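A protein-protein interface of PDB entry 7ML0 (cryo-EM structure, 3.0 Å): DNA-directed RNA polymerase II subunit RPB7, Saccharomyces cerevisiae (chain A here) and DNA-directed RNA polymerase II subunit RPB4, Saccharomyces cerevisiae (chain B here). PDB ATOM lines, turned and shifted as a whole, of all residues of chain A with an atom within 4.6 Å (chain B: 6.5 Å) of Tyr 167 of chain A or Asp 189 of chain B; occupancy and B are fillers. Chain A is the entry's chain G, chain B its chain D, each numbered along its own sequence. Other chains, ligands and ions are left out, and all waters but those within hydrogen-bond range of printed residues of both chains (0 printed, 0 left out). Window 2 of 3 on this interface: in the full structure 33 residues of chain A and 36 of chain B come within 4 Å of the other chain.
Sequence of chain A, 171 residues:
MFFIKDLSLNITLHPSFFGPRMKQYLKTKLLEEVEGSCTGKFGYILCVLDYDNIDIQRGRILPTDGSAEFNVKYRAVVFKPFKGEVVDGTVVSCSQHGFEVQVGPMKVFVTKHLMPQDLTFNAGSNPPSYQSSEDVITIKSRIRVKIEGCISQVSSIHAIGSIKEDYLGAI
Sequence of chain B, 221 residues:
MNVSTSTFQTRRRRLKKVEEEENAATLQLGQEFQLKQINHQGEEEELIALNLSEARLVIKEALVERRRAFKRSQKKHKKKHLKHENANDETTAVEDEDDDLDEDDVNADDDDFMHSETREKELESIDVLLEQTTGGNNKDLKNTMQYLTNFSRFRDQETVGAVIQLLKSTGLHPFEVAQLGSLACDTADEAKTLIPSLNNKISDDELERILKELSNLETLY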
ATOM      1  N   ARG A 144     -10.736   2.992 -24.477  1.00  0.00           N
ATOM      2  CA  ARG A 144      -9.515   3.510 -23.878  1.00  0.00           C
ATOM      3  C   ARG A 144      -8.334   2.672 -24.355  1.00  0.00           C
ATOM      4  O   ARG A 144      -8.144   1.544 -23.895  1.00  0.00           O
ATOM      5  CB  ARG A 144      -9.617   3.487 -22.354  1.00  0.00           C
ATOM      6  CG  ARG A 144      -8.384   3.998 -21.651  1.00  0.00           C
ATOM      7  CD  ARG A 144      -8.601   4.064 -20.161  1.00  0.00           C
ATOM      8  NE  ARG A 144      -9.825   4.779 -19.830  1.00  0.00           N
ATOM      9  CZ  ARG A 144     -10.177   5.122 -18.596  1.00  0.00           C
ATOM     10  NH1 ARG A 144      -9.396   4.825 -17.570  1.00  0.00           N
ATOM     11  NH2 ARG A 144     -11.314   5.768 -18.389  1.00  0.00           N
ATOM     12  N   GLU A 165      -5.194  -5.172 -22.081  1.00  0.00           N
ATOM     13  CA  GLU A 165      -5.100  -5.301 -20.637  1.00  0.00           C
ATOM     14  C   GLU A 165      -6.320  -4.690 -19.954  1.00  0.00           C
ATOM     15  O   GLU A 165      -7.329  -4.370 -20.587  1.00  0.00           O
ATOM     16  CB  GLU A 165      -3.789  -4.690 -20.138  1.00  0.00           C
ATOM     17  CG  GLU A 165      -2.534  -5.343 -20.722  1.00  0.00           C
ATOM     18  CD  GLU A 165      -2.394  -5.119 -22.222  1.00  0.00           C
ATOM     19  OE1 GLU A 165      -3.067  -4.219 -22.766  1.00  0.00           O
ATOM     20  OE2 GLU A 165      -1.631  -5.858 -22.866  1.00  0.00           O
ATOM     21  N   ASP A 166      -6.240  -4.566 -18.639  1.00  0.00           N
ATOM     22  CA  ASP A 166      -7.334  -4.061 -17.835  1.00  0.00           C
ATOM     23  C   ASP A 166      -7.477  -2.546 -17.991  1.00  0.00           C
ATOM     24  O   ASP A 166      -6.563  -1.849 -18.439  1.00  0.00           O
ATOM     25  CB  ASP A 166      -7.109  -4.426 -16.375  1.00  0.00           C
ATOM     26  CG  ASP A 166      -5.756  -3.994 -15.885  1.00  0.00           C
ATOM     27  OD1 ASP A 166      -5.034  -3.353 -16.672  1.00  0.00           O
ATOM     28  OD2 ASP A 166      -5.415  -4.291 -14.724  1.00  0.00           O
ATOM     29  N   TYR A 167      -8.640  -2.041 -17.573  1.00  0.00           N
ATOM     30  CA  TYR A 167      -9.055  -0.654 -17.789  1.00  0.00           C
ATOM     31  C   TYR A 167      -9.098  -0.319 -19.269  1.00  0.00           C
ATOM     32  O   TYR A 167      -9.107   0.850 -19.651  1.00  0.00           O
ATOM     33  CB  TYR A 167      -8.159   0.348 -17.055  1.00  0.00           C
ATOM     34  CG  TYR A 167      -7.581  -0.159 -15.767  1.00  0.00           C
ATOM     35  CD1 TYR A 167      -8.319  -0.145 -14.603  1.00  0.00           C
ATOM     36  CD2 TYR A 167      -6.288  -0.647 -15.713  1.00  0.00           C
ATOM     37  CE1 TYR A 167      -7.788  -0.620 -13.426  1.00  0.00           C
ATOM     38  CE2 TYR A 167      -5.757  -1.122 -14.547  1.00  0.00           C
ATOM     39  CZ  TYR A 167      -6.511  -1.114 -13.408  1.00  0.00           C
ATOM     40  OH  TYR A 167      -5.972  -1.576 -12.241  1.00  0.00           O
ATOM     41  N   LEU A 168      -9.139  -1.338 -20.119  1.00  0.00           N
ATOM     42  CA  LEU A 168      -9.050  -1.106 -21.550  1.00  0.00           C
ATOM     43  C   LEU A 168     -10.285  -1.644 -22.250  1.00  0.00           C
ATOM     44  O   LEU A 168     -11.252  -2.036 -21.593  1.00  0.00           O
ATOM     45  CB  LEU A 168      -7.778  -1.737 -22.102  1.00  0.00           C
ATOM     46  CG  LEU A 168      -6.508  -1.203 -21.428  1.00  0.00           C
ATOM     47  CD1 LEU A 168      -5.250  -1.853 -21.985  1.00  0.00           C
ATOM     48  CD2 LEU A 168      -6.425   0.316 -21.524  1.00  0.00           C
ATOM     49  N   CYS B 185      -9.971   8.021 -14.439  1.00  0.00           N
ATOM     50  CA  CYS B 185      -9.340   7.017 -13.594  1.00  0.00           C
ATOM     51  C   CYS B 185     -10.215   6.761 -12.369  1.00  0.00           C
ATOM     52  O   CYS B 185     -10.294   7.606 -11.472  1.00  0.00           O
ATOM     53  CB  CYS B 185      -7.949   7.491 -13.189  1.00  0.00           C
ATOM     54  SG  CYS B 185      -6.811   6.206 -12.649  1.00  0.00           S
ATOM     55  N   THR B 187      -9.955   3.523 -10.497  1.00  0.00           N
ATOM     56  CA  THR B 187      -9.105   2.762  -9.599  1.00  0.00           C
ATOM     57  C   THR B 187      -7.743   3.419  -9.464  1.00  0.00           C
ATOM     58  O   THR B 187      -7.334   4.225 -10.300  1.00  0.00           O
ATOM     59  CB  THR B 187      -8.929   1.335 -10.108  1.00  0.00           C
ATOM     60  OG1 THR B 187      -7.558   1.129 -10.462  1.00  0.00           O
ATOM     61  CG2 THR B 187      -9.800   1.113 -11.330  1.00  0.00           C
ATOM     62  N   ALA B 188      -7.040   3.072  -8.384  1.00  0.00           N
ATOM     63  CA  ALA B 188      -5.643   3.456  -8.238  1.00  0.00           C
ATOM     64  C   ALA B 188      -4.691   2.375  -8.713  1.00  0.00           C
ATOM     65  O   ALA B 188      -3.544   2.682  -9.058  1.00  0.00           O
ATOM     66  CB  ALA B 188      -5.329   3.807  -6.789  1.00  0.00           C
ATOM     67  N   ASP B 189      -5.139   1.123  -8.737  1.00  0.00           N
ATOM     68  CA  ASP B 189      -4.447   0.105  -9.514  1.00  0.00           C
ATOM     69  C   ASP B 189      -4.403   0.497 -10.984  1.00  0.00           C
ATOM     70  O   ASP B 189      -3.508   0.069 -11.720  1.00  0.00           O
ATOM     71  CB  ASP B 189      -5.153  -1.241  -9.313  1.00  0.00           C
ATOM     72  CG  ASP B 189      -4.404  -2.408  -9.924  1.00  0.00           C
ATOM     73  OD1 ASP B 189      -4.247  -2.449 -11.162  1.00  0.00           O
ATOM     74  OD2 ASP B 189      -3.984  -3.300  -9.160  1.00  0.00           O
ATOM     75  N   GLU B 190      -5.357   1.324 -11.412  1.00  0.00           N
ATOM     76  CA  GLU B 190      -5.421   1.780 -12.794  1.00  0.00           C
ATOM     77  C   GLU B 190      -4.091   2.361 -13.250  1.00  0.00           C
ATOM     78  O   GLU B 190      -3.476   1.860 -14.198  1.00  0.00           O
ATOM     79  CB  GLU B 190      -6.546   2.805 -12.917  1.00  0.00           C
ATOM     80  CG  GLU B 190      -7.122   3.039 -14.291  1.00  0.00           C
ATOM     81  CD  GLU B 190      -8.443   3.788 -14.210  1.00  0.00           C
ATOM     82  OE1 GLU B 190      -8.965   3.919 -13.083  1.00  0.00           O
ATOM     83  OE2 GLU B 190      -8.953   4.250 -15.252  1.00  0.00           O
ATOM     84  N   ALA B 191      -3.609   3.393 -12.548  1.00  0.00           N
ATOM     85  CA  ALA B 191      -2.407   4.096 -12.988  1.00  0.00           C
ATOM     86  C   ALA B 191      -1.231   3.148 -13.129  1.00  0.00           C
ATOM     87  O   ALA B 191      -0.630   3.050 -14.205  1.00  0.00           O
ATOM     88  CB  ALA B 191      -2.062   5.213 -12.008  1.00  0.00           C
ATOM     89  N   LYS B 192      -0.929   2.396 -12.073  1.00  0.00           N
ATOM     90  CA  LYS B 192       0.197   1.478 -12.123  1.00  0.00           C
ATOM     91  C   LYS B 192       0.006   0.391 -13.170  1.00  0.00           C
ATOM     92  O   LYS B 192       0.936  -0.377 -13.424  1.00  0.00           O
ATOM     93  CB  LYS B 192       0.415   0.850 -10.752  1.00  0.00           C
ATOM     94  CG  LYS B 192       0.050   1.761  -9.602  1.00  0.00           C
ATOM     95  CD  LYS B 192       0.020   1.017  -8.281  1.00  0.00           C
ATOM     96  CE  LYS B 192      -1.247   0.185  -8.118  1.00  0.00           C
ATOM     97  NZ  LYS B 192      -1.314  -1.047  -8.962  1.00  0.00           N
ATOM     98  N   THR B 193      -1.171   0.300 -13.778  1.00  0.00           N
ATOM     99  CA  THR B 193      -1.343  -0.538 -14.954  1.00  0.00           C
ATOM    100  C   THR B 193      -1.610   0.257 -16.219  1.00  0.00           C
ATOM    101  O   THR B 193      -1.205  -0.168 -17.298  1.00  0.00           O
ATOM    102  CB  THR B 193      -2.481  -1.535 -14.744  1.00  0.00           C
ATOM    103  OG1 THR B 193      -2.534  -1.921 -13.363  1.00  0.00           O
ATOM    104  CG2 THR B 193      -2.253  -2.771 -15.600  1.00  0.00           C
ATOM    105  N   LEU B 194      -2.287   1.401 -16.123  1.00  0.00           N
ATOM    106  CA  LEU B 194      -2.554   2.186 -17.323  1.00  0.00           C
ATOM    107  C   LEU B 194      -1.340   2.995 -17.732  1.00  0.00           C
ATOM    108  O   LEU B 194      -0.971   3.027 -18.912  1.00  0.00           O
ATOM    109  CB  LEU B 194      -3.742   3.114 -17.099  1.00  0.00           C
ATOM    110  CG  LEU B 194      -5.126   2.519 -17.310  1.00  0.00           C
ATOM    111  CD1 LEU B 194      -6.088   3.627 -17.670  1.00  0.00           C
ATOM    112  CD2 LEU B 194      -5.082   1.462 -18.391  1.00  0.00           C
ATOM    113  N   ASP B 204      -1.113   4.540  -4.285  1.00  0.00           N
ATOM    114  CA  ASP B 204      -2.553   4.546  -4.489  1.00  0.00           C
ATOM    115  C   ASP B 204      -3.263   5.455  -3.499  1.00  0.00           C
ATOM    116  O   ASP B 204      -4.328   5.995  -3.807  1.00  0.00           O
ATOM    117  CB  ASP B 204      -3.065   3.113  -4.392  1.00  0.00           C
ATOM    118  CG  ASP B 204      -2.456   2.219  -5.449  1.00  0.00           C
ATOM    119  OD1 ASP B 204      -2.468   2.605  -6.630  1.00  0.00           O
ATOM    120  OD2 ASP B 204      -1.944   1.139  -5.103  1.00  0.00           O
ATOM    121  N   LEU B 207      -2.586   8.890  -4.714  1.00  0.00           N
ATOM    122  CA  LEU B 207      -3.254   8.780  -6.000  1.00  0.00           C
ATOM    123  C   LEU B 207      -4.757   8.880  -5.822  1.00  0.00           C
ATOM    124  O   LEU B 207      -5.393   9.833  -6.283  1.00  0.00           O
ATOM    125  CB  LEU B 207      -2.875   7.448  -6.649  1.00  0.00           C
ATOM    126  CG  LEU B 207      -3.238   7.010  -8.070  1.00  0.00           C
ATOM    127  CD1 LEU B 207      -2.600   5.649  -8.355  1.00  0.00           C
ATOM    128  CD2 LEU B 207      -4.727   6.920  -8.297  1.00  0.00           C
ATOM    129  N   GLU B 208      -5.339   7.904  -5.135  1.00  0.00           N
ATOM    130  CA  GLU B 208      -6.784   7.777  -5.179  1.00  0.00           C
ATOM    131  C   GLU B 208      -7.452   8.859  -4.357  1.00  0.00           C
ATOM    132  O   GLU B 208      -8.551   9.306  -4.697  1.00  0.00           O
ATOM    133  CB  GLU B 208      -7.223   6.396  -4.718  1.00  0.00           C
ATOM    134  CG  GLU B 208      -8.350   5.865  -5.556  1.00  0.00           C
ATOM    135  CD  GLU B 208      -8.297   4.376  -5.691  1.00  0.00           C
ATOM    136  OE1 GLU B 208      -7.711   3.729  -4.801  1.00  0.00           O
ATOM    137  OE2 GLU B 208      -8.809   3.853  -6.697  1.00  0.00           O
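The backbone carbonyl oxygen (O) of Asp 189 of chain B sits close to the side-chain hydroxyl (OH) of Tyr 167 of chain A (3.0 Å). OH of Tyr 167 of chain A sits at hydrogen-bond distance from N of Glu 190 of chain B. The side-chain carboxylate (OE2) of Glu 190 of chain B is in salt-bridge range of the guanidinium group (NH1) of Arg 144 of chain A, 2.4 Å away.
The side-chain amino group of Lys 192 of chain B lies within salt-bridge range of the side-chain carboxylate of Asp 189 of chain B, at 3.5 Å. The side-chain hydroxyl (OG1) of Thr 187 of chain B lies within hydrogen-bond range of the backbone NH (N) of Asp 189 of chain B. OG1 of Thr 187 of chain B is in hydrogen-bond range of N of Glu 190 of chain B (2.4 Å). O of Asp 189 of chain B lies within hydrogen-bond range of OG1 of Thr 193 of chain B, at 2.8 Å. SG of Cys 185 of chain B sits close to OE1 of Glu 190 of chain B (3.2 Å). The backbone carbonyl oxygen (O) of Thr 187 of chain B lies within hydrogen-bond range of the side-chain sulfur (SG) of Cys 185 of chain B (3.1 Å).
Arg 144 of chain A touches Leu 194 of chain B (NH1 to CD1, 3.5 Å). Asp 166 of chain A touches Thr 193 of chain B. CD2 of Leu 194 of chain B touches O of Asp 166 of chain A, 3.6 Å away. CE1 of Tyr 167 of chain A touches CG2 of Thr 187 of chain B, 3.4 Å away. Tyr 167 of chain A touches Thr 193 of chain B (CE2 to CB, 3.3 Å). Leu 194 of chain B touches Tyr 167 of chain A (CD2 to CB, 3.5 Å). Leu 168 of chain A touches Leu 194 of chain B.
Of the printed residues of chain B, Arg 144 of chain A touches Glu 190 and Leu 194. Tyr 167 of chain A touches five residues of chain B. Of the printed residues of chain B, Leu 168 of chain A touches Leu 194. Asp 189 of chain B touches just one residue of chain A: Tyr 167 (2.2 Å). Ala 191 of chain B touches none of the printed residues of chain A. Of the printed residues of chain A, Thr 193 of chain B touches Asp 166 and Tyr 167. The nearest residue of chain A that does not touch Asp 189 of chain B is Asp 166 of chain A (4.2 Å). The nearest printed residue of chain A that does not touch Glu 190 of chain B is Asp 166 of chain A (6.0 Å).
Of the 5 printed residues of chain A, 4 touch a printed residue of chain B. Hydrophobic or aromatic side chains of chain B within 4 Å of the printed part of chain A: Leu 194. Among the printed residues, 10 pairs touch across the chains.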
